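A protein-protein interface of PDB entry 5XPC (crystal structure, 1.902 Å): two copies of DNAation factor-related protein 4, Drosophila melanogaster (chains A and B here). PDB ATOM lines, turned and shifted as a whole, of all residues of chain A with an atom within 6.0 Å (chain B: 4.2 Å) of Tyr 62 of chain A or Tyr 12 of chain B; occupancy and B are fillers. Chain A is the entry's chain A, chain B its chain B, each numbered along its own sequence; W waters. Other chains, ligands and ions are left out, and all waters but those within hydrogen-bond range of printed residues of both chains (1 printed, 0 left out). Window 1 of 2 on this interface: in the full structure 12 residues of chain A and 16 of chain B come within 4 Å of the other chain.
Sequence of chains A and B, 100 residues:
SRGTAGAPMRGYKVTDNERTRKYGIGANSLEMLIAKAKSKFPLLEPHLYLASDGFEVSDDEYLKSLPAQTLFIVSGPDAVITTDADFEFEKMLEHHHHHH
Water W1 lies within hydrogen-bond range of O of Ser 65 of chain A and NE2 of Gln 69 of chain B.
N of Gly 24 of chain B is in hydrogen-bond range of O of Glu 56 of chain A (2.7 Å). The backbone carbonyl oxygen (O) of Gly 24 of chain B lies within hydrogen-bond range of the side-chain hydroxyl (OG) of Ser 58 of chain A (2.7 Å). OD1 of Asp 59 of chain A is in hydrogen-bond range of N of Gly 26 of chain B, 3.3 Å away. The side-chain hydroxyl of Tyr 62 of chain A lies within hydrogen-bond range of the side-chain amide oxygen of Gln 69 of chain B. OG of Ser 65 of chain A is in hydrogen-bond range of NE2 of Gln 69 of chain B (3.2 Å).
Position printed for both chains: 63.
N of Glu 61 of chain A lies close to OD1 of Asp 59 of chain A (3.5 Å). The backbone carbonyl oxygen (O) of Tyr 62 of chain A is in hydrogen-bond range of the side-chain hydroxyl (OG) of Ser 65 of chain A. O of Gly 11 of chain B is in hydrogen-bond range of N of Gln 69 of chain B (2.7 Å). O of Tyr 12 of chain B lies within hydrogen-bond range of N of Ile 25 of chain B, at 2.8 Å. The backbone carbonyl oxygen (O) of Thr 70 of chain B is in hydrogen-bond range of the backbone NH (N) of Lys 13 of chain B. The backbone carbonyl oxygen (O) of Lys 13 of chain B sits at hydrogen-bond distance from the backbone NH (N) of Phe 72 of chain B, at 2.7 Å.
Lys 13 of chain B touches Leu 50 of chain A (NZ to CD1, 3.9 Å). CB of Lys 13 of chain B touches CE2 of Phe 55 of chain A (3.6 Å). Tyr 23 of chain B touches Phe 55 of chain A (N to CD2, 3.5 Å). Ile 25 of chain B touches Ser 58 of chain A. O of Tyr 12 of chain B touches CE1 of Tyr 62 of chain A (3.4 Å). Lys 13 of chain B touches Tyr 62 of chain A. Gly 24 of chain B touches Tyr 62 of chain A. Gly 26 of chain B touches Tyr 62 of chain A. Ser 65 of chain A touches Gly 11 of chain B. Leu 66 of chain A touches Gln 69 of chain B (CD2 to NE2, 3.97 Å).
Tyr 62 of chain A touches just these residues of chain B: Gly 11, Tyr 12, Lys 13, Gly 24, Ile 25, Gly 26 and Gln 69. Tyr 12 of chain B touches one residue of chain A. Printed residues of chain A within 4 Å of Ile 25 of chain B: Ser 58 and Tyr 62. Printed residues of chain B within 4 Å of Leu 66 of chain A: Gln 69 (3.97 Å). The nearest residue of chain A that does not touch Tyr 12 of chain B is Ser 65 of chain A (5.4 Å). The nearest printed residue of chain A that does not touch Lys 13 of chain B is Leu 66 of chain A (6.2 Å).
Of the 14 printed residues of chain B, 8 touch a printed residue of chain A. Among the printed residues, no Asp or Glu carboxylate lies within 4 Å of a Lys or Arg side-chain nitrogen of the other chain.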
ATOM      1  N   LEU A  50      18.133  19.478 -23.890  1.00  0.00           N
ATOM      2  CA  LEU A  50      17.006  18.549 -24.007  1.00  0.00           C
ATOM      3  C   LEU A  50      17.220  17.597 -25.177  1.00  0.00           C
ATOM      4  O   LEU A  50      17.528  18.027 -26.294  1.00  0.00           O
ATOM      5  CB  LEU A  50      15.692  19.307 -24.198  1.00  0.00           C
ATOM      6  CG  LEU A  50      15.226  20.176 -23.037  1.00  0.00           C
ATOM      7  CD1 LEU A  50      13.866  20.792 -23.385  1.00  0.00           C
ATOM      8  CD2 LEU A  50      15.138  19.379 -21.758  1.00  0.00           C
ATOM      9  N   PHE A  55      17.165  22.219 -26.696  1.00  0.00           N
ATOM     10  CA  PHE A  55      17.262  23.473 -25.962  1.00  0.00           C
ATOM     11  C   PHE A  55      18.154  23.293 -24.741  1.00  0.00           C
ATOM     12  O   PHE A  55      18.053  22.295 -24.017  1.00  0.00           O
ATOM     13  CB  PHE A  55      15.870  23.990 -25.591  1.00  0.00           C
ATOM     14  CG  PHE A  55      15.238  24.772 -26.702  1.00  0.00           C
ATOM     15  CD1 PHE A  55      14.844  24.133 -27.870  1.00  0.00           C
ATOM     16  CD2 PHE A  55      15.113  26.159 -26.621  1.00  0.00           C
ATOM     17  CE1 PHE A  55      14.308  24.856 -28.928  1.00  0.00           C
ATOM     18  CE2 PHE A  55      14.582  26.886 -27.679  1.00  0.00           C
ATOM     19  CZ  PHE A  55      14.184  26.235 -28.834  1.00  0.00           C
ATOM     20  N   GLU A  56      19.079  24.228 -24.556  1.00  0.00           N
ATOM     21  CA  GLU A  56      20.062  24.103 -23.490  1.00  0.00           C
ATOM     22  C   GLU A  56      19.439  24.503 -22.163  1.00  0.00           C
ATOM     23  O   GLU A  56      18.698  25.486 -22.081  1.00  0.00           O
ATOM     24  CB  GLU A  56      21.293  24.977 -23.774  1.00  0.00           C
ATOM     25  CG  GLU A  56      22.317  24.912 -22.634  1.00  0.00           C
ATOM     26  CD  GLU A  56      23.549  25.753 -22.863  1.00  0.00           C
ATOM     27  OE1 GLU A  56      23.797  26.153 -24.019  1.00  0.00           O
ATOM     28  OE2 GLU A  56      24.278  26.003 -21.875  1.00  0.00           O
ATOM     29  N   VAL A  57      19.741  23.738 -21.117  1.00  0.00           N
ATOM     30  CA  VAL A  57      19.255  24.038 -19.772  1.00  0.00           C
ATOM     31  C   VAL A  57      20.132  25.168 -19.240  1.00  0.00           C
ATOM     32  O   VAL A  57      21.252  24.935 -18.779  1.00  0.00           O
ATOM     33  CB  VAL A  57      19.296  22.806 -18.868  1.00  0.00           C
ATOM     34  CG1 VAL A  57      18.749  23.133 -17.489  1.00  0.00           C
ATOM     35  CG2 VAL A  57      18.496  21.675 -19.499  1.00  0.00           C
ATOM     36  N   SER A  58      19.640  26.406 -19.325  1.00  0.00           N
ATOM     37  CA  SER A  58      20.512  27.548 -19.071  1.00  0.00           C
ATOM     38  C   SER A  58      20.623  27.914 -17.595  1.00  0.00           C
ATOM     39  O   SER A  58      21.611  28.551 -17.207  1.00  0.00           O
ATOM     40  CB  SER A  58      20.049  28.774 -19.872  1.00  0.00           C
ATOM     41  OG  SER A  58      18.954  29.434 -19.242  1.00  0.00           O
ATOM     42  N   ASP A  59      19.658  27.534 -16.759  1.00  0.00           N
ATOM     43  CA  ASP A  59      19.745  27.897 -15.350  1.00  0.00           C
ATOM     44  C   ASP A  59      18.942  26.901 -14.525  1.00  0.00           C
ATOM     45  O   ASP A  59      18.176  26.089 -15.052  1.00  0.00           O
ATOM     46  CB  ASP A  59      19.287  29.352 -15.096  1.00  0.00           C
ATOM     47  CG  ASP A  59      17.882  29.657 -15.625  1.00  0.00           C
ATOM     48  OD1 ASP A  59      17.037  28.749 -15.693  1.00  0.00           O
ATOM     49  OD2 ASP A  59      17.611  30.836 -15.960  1.00  0.00           O
ATOM     50  N   ASP A  60      19.158  26.969 -13.209  1.00  0.00           N
ATOM     51  CA  ASP A  60      18.495  26.054 -12.285  1.00  0.00           C
ATOM     52  C   ASP A  60      16.984  26.202 -12.358  1.00  0.00           C
ATOM     53  O   ASP A  60      16.255  25.210 -12.259  1.00  0.00           O
ATOM     54  CB  ASP A  60      18.995  26.307 -10.865  1.00  0.00           C
ATOM     55  CG  ASP A  60      18.538  25.249  -9.884  1.00  0.00           C
ATOM     56  OD1 ASP A  60      18.796  24.051 -10.131  1.00  0.00           O
ATOM     57  OD2 ASP A  60      17.909  25.613  -8.870  1.00  0.00           O
ATOM     58  N   GLU A  61      16.492  27.436 -12.543  1.00  0.00           N
ATOM     59  CA  GLU A  61      15.049  27.634 -12.625  1.00  0.00           C
ATOM     60  C   GLU A  61      14.449  26.861 -13.795  1.00  0.00           C
ATOM     61  O   GLU A  61      13.357  26.289 -13.676  1.00  0.00           O
ATOM     62  CB  GLU A  61      14.727  29.127 -12.732  1.00  0.00           C
ATOM     63  CG  GLU A  61      15.109  29.925 -11.490  1.00  0.00           C
ATOM     64  CD  GLU A  61      16.611  30.216 -11.376  1.00  0.00           C
ATOM     65  OE1 GLU A  61      17.344  30.096 -12.383  1.00  0.00           O
ATOM     66  OE2 GLU A  61      17.056  30.577 -10.269  1.00  0.00           O
ATOM     67  N   TYR A  62      15.145  26.814 -14.931  1.00  0.00           N
ATOM     68  CA  TYR A  62      14.633  26.016 -16.038  1.00  0.00           C
ATOM     69  C   TYR A  62      14.661  24.532 -15.696  1.00  0.00           C
ATOM     70  O   TYR A  62      13.689  23.811 -15.961  1.00  0.00           O
ATOM     71  CB  TYR A  62      15.418  26.276 -17.333  1.00  0.00           C
ATOM     72  CG  TYR A  62      14.721  25.593 -18.481  1.00  0.00           C
ATOM     73  CD1 TYR A  62      13.510  26.086 -18.969  1.00  0.00           C
ATOM     74  CD2 TYR A  62      15.223  24.415 -19.027  1.00  0.00           C
ATOM     75  CE1 TYR A  62      12.837  25.439 -19.996  1.00  0.00           C
ATOM     76  CE2 TYR A  62      14.558  23.763 -20.052  1.00  0.00           C
ATOM     77  CZ  TYR A  62      13.362  24.271 -20.524  1.00  0.00           C
ATOM     78  OH  TYR A  62      12.694  23.621 -21.539  1.00  0.00           O
ATOM     79  N   LEU A  63      15.761  24.061 -15.107  1.00  0.00           N
ATOM     80  CA  LEU A  63      15.849  22.653 -14.721  1.00  0.00           C
ATOM     81  C   LEU A  63      14.655  22.256 -13.858  1.00  0.00           C
ATOM     82  O   LEU A  63      13.995  21.241 -14.110  1.00  0.00           O
ATOM     83  CB  LEU A  63      17.158  22.393 -13.977  1.00  0.00           C
ATOM     84  CG  LEU A  63      17.286  20.942 -13.479  1.00  0.00           C
ATOM     85  CD1 LEU A  63      17.317  19.985 -14.666  1.00  0.00           C
ATOM     86  CD2 LEU A  63      18.506  20.756 -12.610  1.00  0.00           C
ATOM     87  N   LYS A  64      14.337  23.081 -12.859  1.00  0.00           N
ATOM     88  CA  LYS A  64      13.258  22.748 -11.936  1.00  0.00           C
ATOM     89  C   LYS A  64      11.890  22.798 -12.604  1.00  0.00           C
ATOM     90  O   LYS A  64      10.938  22.222 -12.070  1.00  0.00           O
ATOM     91  CB  LYS A  64      13.290  23.689 -10.719  1.00  0.00           C
ATOM     92  CG  LYS A  64      14.621  23.703  -9.951  1.00  0.00           C
ATOM     93  CD  LYS A  64      14.992  22.336  -9.414  1.00  0.00           C
ATOM     94  CE  LYS A  64      16.412  22.306  -8.848  1.00  0.00           C
ATOM     95  NZ  LYS A  64      16.615  23.223  -7.685  1.00  0.00           N
ATOM     96  N   SER A  65      11.763  23.468 -13.756  1.00  0.00           N
ATOM     97  CA  SER A  65      10.508  23.449 -14.498  1.00  0.00           C
ATOM     98  C   SER A  65      10.289  22.148 -15.264  1.00  0.00           C
ATOM     99  O   SER A  65       9.193  21.939 -15.801  1.00  0.00           O
ATOM    100  CB  SER A  65      10.453  24.626 -15.483  1.00  0.00           C
ATOM    101  OG  SER A  65      11.187  24.329 -16.661  1.00  0.00           O
ATOM    102  N   LEU A  66      11.302  21.269 -15.332  1.00  0.00           N
ATOM    103  CA  LEU A  66      11.177  20.055 -16.126  1.00  0.00           C
ATOM    104  C   LEU A  66      10.712  18.888 -15.256  1.00  0.00           C
ATOM    105  O   LEU A  66      10.965  18.869 -14.049  1.00  0.00           O
ATOM    106  CB  LEU A  66      12.516  19.702 -16.765  1.00  0.00           C
ATOM    107  CG  LEU A  66      13.062  20.785 -17.705  1.00  0.00           C
ATOM    108  CD1 LEU A  66      14.485  20.442 -18.107  1.00  0.00           C
ATOM    109  CD2 LEU A  66      12.158  20.895 -18.937  1.00  0.00           C
ATOM    110  N   ARG B  10       8.500  29.992 -14.061  1.00  0.00           N
ATOM    111  CA  ARG B  10       8.057  29.069 -15.093  1.00  0.00           C
ATOM    112  C   ARG B  10       9.173  28.888 -16.110  1.00  0.00           C
ATOM    113  O   ARG B  10      10.031  29.756 -16.275  1.00  0.00           O
ATOM    114  CB  ARG B  10       6.787  29.560 -15.791  1.00  0.00           C
ATOM    115  CG  ARG B  10       5.648  29.862 -14.829  1.00  0.00           C
ATOM    116  CD  ARG B  10       4.545  30.594 -15.557  1.00  0.00           C
ATOM    117  NE  ARG B  10       3.681  29.662 -16.264  1.00  0.00           N
ATOM    118  CZ  ARG B  10       3.095  29.914 -17.430  1.00  0.00           C
ATOM    119  NH1 ARG B  10       3.293  31.072 -18.051  1.00  0.00           N
ATOM    120  NH2 ARG B  10       2.310  28.999 -17.976  1.00  0.00           N
ATOM    121  N   GLY B  11       9.157  27.741 -16.785  1.00  0.00           N
ATOM    122  CA  GLY B  11      10.130  27.459 -17.826  1.00  0.00           C
ATOM    123  C   GLY B  11       9.628  27.905 -19.191  1.00  0.00           C
ATOM    124  O   GLY B  11       8.472  27.677 -19.546  1.00  0.00           O
ATOM    125  N   TYR B  12      10.524  28.534 -19.956  1.00  0.00           N
ATOM    126  CA  TYR B  12      10.234  29.004 -21.311  1.00  0.00           C
ATOM    127  C   TYR B  12      11.399  28.651 -22.228  1.00  0.00           C
ATOM    128  O   TYR B  12      12.511  28.374 -21.768  1.00  0.00           O
ATOM    129  CB  TYR B  12       9.992  30.528 -21.352  1.00  0.00           C
ATOM    130  CG  TYR B  12       8.885  31.035 -20.434  1.00  0.00           C
ATOM    131  CD1 TYR B  12       9.183  31.660 -19.226  1.00  0.00           C
ATOM    132  CD2 TYR B  12       7.543  30.899 -20.785  1.00  0.00           C
ATOM    133  CE1 TYR B  12       8.167  32.135 -18.386  1.00  0.00           C
ATOM    134  CE2 TYR B  12       6.525  31.376 -19.955  1.00  0.00           C
ATOM    135  CZ  TYR B  12       6.841  31.989 -18.761  1.00  0.00           C
ATOM    136  OH  TYR B  12       5.823  32.459 -17.941  1.00  0.00           O
ATOM    137  N   LYS B  13      11.153  28.679 -23.540  1.00  0.00           N
ATOM    138  CA  LYS B  13      12.194  28.420 -24.527  1.00  0.00           C
ATOM    139  C   LYS B  13      12.372  29.648 -25.410  1.00  0.00           C
ATOM    140  O   LYS B  13      11.382  30.241 -25.858  1.00  0.00           O
ATOM    141  CB  LYS B  13      11.864  27.192 -25.380  1.00  0.00           C
ATOM    142  CG  LYS B  13      11.820  25.905 -24.553  1.00  0.00           C
ATOM    143  CD  LYS B  13      11.336  24.716 -25.369  1.00  0.00           C
ATOM    144  CE  LYS B  13      11.205  23.476 -24.497  1.00  0.00           C
ATOM    145  NZ  LYS B  13      10.857  22.297 -25.338  1.00  0.00           N
ATOM    146  N   TYR B  23      17.848  28.136 -25.887  1.00  0.00           N
ATOM    147  CA  TYR B  23      17.977  28.114 -24.439  1.00  0.00           C
ATOM    148  C   TYR B  23      16.627  27.891 -23.784  1.00  0.00           C
ATOM    149  O   TYR B  23      15.636  28.529 -24.156  1.00  0.00           O
ATOM    150  CB  TYR B  23      18.577  29.413 -23.911  1.00  0.00           C
ATOM    151  CG  TYR B  23      19.955  29.676 -24.437  1.00  0.00           C
ATOM    152  CD1 TYR B  23      20.154  30.515 -25.531  1.00  0.00           C
ATOM    153  CD2 TYR B  23      21.063  29.066 -23.861  1.00  0.00           C
ATOM    154  CE1 TYR B  23      21.428  30.751 -26.021  1.00  0.00           C
ATOM    155  CE2 TYR B  23      22.335  29.302 -24.343  1.00  0.00           C
ATOM    156  CZ  TYR B  23      22.511  30.144 -25.424  1.00  0.00           C
ATOM    157  OH  TYR B  23      23.782  30.376 -25.910  1.00  0.00           O
ATOM    158  N   GLY B  24      16.598  26.989 -22.805  1.00  0.00           N
ATOM    159  CA  GLY B  24      15.507  26.948 -21.849  1.00  0.00           C
ATOM    160  C   GLY B  24      15.868  27.888 -20.716  1.00  0.00           C
ATOM    161  O   GLY B  24      16.998  27.866 -20.220  1.00  0.00           O
ATOM    162  N   ILE B  25      14.913  28.728 -20.326  1.00  0.00           N
ATOM    163  CA  ILE B  25      15.132  29.802 -19.362  1.00  0.00           C
ATOM    164  C   ILE B  25      13.978  29.820 -18.372  1.00  0.00           C
ATOM    165  O   ILE B  25      12.810  29.824 -18.777  1.00  0.00           O
ATOM    166  CB  ILE B  25      15.233  31.173 -20.060  1.00  0.00           C
ATOM    167  CG1 ILE B  25      16.433  31.204 -21.017  1.00  0.00           C
ATOM    168  CG2 ILE B  25      15.310  32.290 -19.032  1.00  0.00           C
ATOM    169  CD1 ILE B  25      16.507  32.510 -21.828  1.00  0.00           C
ATOM    170  N   GLY B  26      14.301  29.880 -17.081  1.00  0.00           N
ATOM    171  CA  GLY B  26      13.285  30.064 -16.052  1.00  0.00           C
ATOM    172  C   GLY B  26      13.104  31.538 -15.722  1.00  0.00           C
ATOM    173  O   GLY B  26      14.075  32.278 -15.564  1.00  0.00           O
ATOM    174  N   ALA B  27      11.844  31.964 -15.640  1.00  0.00           N
ATOM    175  CA  ALA B  27      11.566  33.351 -15.303  1.00  0.00           C
ATOM    176  C   ALA B  27      10.204  33.470 -14.635  1.00  0.00           C
ATOM    177  O   ALA B  27       9.296  32.663 -14.874  1.00  0.00           O
ATOM    178  CB  ALA B  27      11.627  34.264 -16.546  1.00  0.00           C
ATOM    179  N   LEU B  33      12.473  37.526 -18.094  1.00  0.00           N
ATOM    180  CA  LEU B  33      12.721  36.656 -19.239  1.00  0.00           C
ATOM    181  C   LEU B  33      13.496  37.392 -20.318  1.00  0.00           C
ATOM    182  O   LEU B  33      14.419  36.832 -20.923  1.00  0.00           O
ATOM    183  CB  LEU B  33      11.409  36.117 -19.809  1.00  0.00           C
ATOM    184  CG  LEU B  33      11.527  35.128 -20.974  1.00  0.00           C
ATOM    185  CD1 LEU B  33      12.527  34.004 -20.648  1.00  0.00           C
ATOM    186  CD2 LEU B  33      10.151  34.520 -21.303  1.00  0.00           C
ATOM    187  N   LEU B  63       2.343  37.123 -21.240  1.00  0.00           N
ATOM    188  CA  LEU B  63       3.322  36.060 -21.006  1.00  0.00           C
ATOM    189  C   LEU B  63       2.764  34.995 -20.069  1.00  0.00           C
ATOM    190  O   LEU B  63       2.862  33.790 -20.335  1.00  0.00           O
ATOM    191  CB  LEU B  63       4.617  36.634 -20.427  1.00  0.00           C
ATOM    192  CG  LEU B  63       5.613  35.544 -19.984  1.00  0.00           C
ATOM    193  CD1 LEU B  63       6.131  34.805 -21.193  1.00  0.00           C
ATOM    194  CD2 LEU B  63       6.795  36.118 -19.209  1.00  0.00           C
ATOM    195  N   GLN B  69       6.810  26.391 -21.261  1.00  0.00           N
ATOM    196  CA  GLN B  69       7.593  25.829 -22.363  1.00  0.00           C
ATOM    197  C   GLN B  69       7.207  26.384 -23.733  1.00  0.00           C
ATOM    198  O   GLN B  69       7.656  25.847 -24.755  1.00  0.00           O
ATOM    199  CB  GLN B  69       7.521  24.294 -22.390  1.00  0.00           C
ATOM    200  CG  GLN B  69       7.857  23.652 -21.050  1.00  0.00           C
ATOM    201  CD  GLN B  69       9.295  23.913 -20.625  1.00  0.00           C
ATOM    202  OE1 GLN B  69      10.163  24.139 -21.462  1.00  0.00           O
ATOM    203  NE2 GLN B  69       9.551  23.871 -19.318  1.00  0.00           N
ATOM    204  N   THR B  70       6.407  27.450 -23.793  1.00  0.00           N
ATOM    205  CA  THR B  70       6.191  28.154 -25.056  1.00  0.00           C
ATOM    206  C   THR B  70       7.526  28.633 -25.625  1.00  0.00           C
ATOM    207  O   THR B  70       8.418  29.041 -24.879  1.00  0.00           O
ATOM    208  CB  THR B  70       5.242  29.342 -24.842  1.00  0.00           C
ATOM    209  OG1 THR B  70       3.924  28.863 -24.528  1.00  0.00           O
ATOM    210  CG2 THR B  70       5.155  30.234 -26.092  1.00  0.00           C
ATOM    211  N   PHE B  72       9.755  31.232 -27.835  1.00  0.00           N
ATOM    212  CA  PHE B  72       9.826  32.625 -28.255  1.00  0.00           C
ATOM    213  C   PHE B  72      11.042  32.855 -29.143  1.00  0.00           C
ATOM    214  O   PHE B  72      12.087  32.221 -28.965  1.00  0.00           O
ATOM    215  CB  PHE B  72       9.907  33.581 -27.047  1.00  0.00           C
ATOM    216  CG  PHE B  72       8.781  33.410 -26.064  1.00  0.00           C
ATOM    217  CD1 PHE B  72       7.521  33.902 -26.350  1.00  0.00           C
ATOM    218  CD2 PHE B  72       8.988  32.764 -24.854  1.00  0.00           C
ATOM    219  CE1 PHE B  72       6.465  33.733 -25.447  1.00  0.00           C
ATOM    220  CE2 PHE B  72       7.944  32.595 -23.951  1.00  0.00           C
ATOM    221  CZ  PHE B  72       6.685  33.085 -24.251  1.00  0.00           C
HETATM  222  O   HOH W   1       7.423  23.568 -17.211  1.00  0.00           O
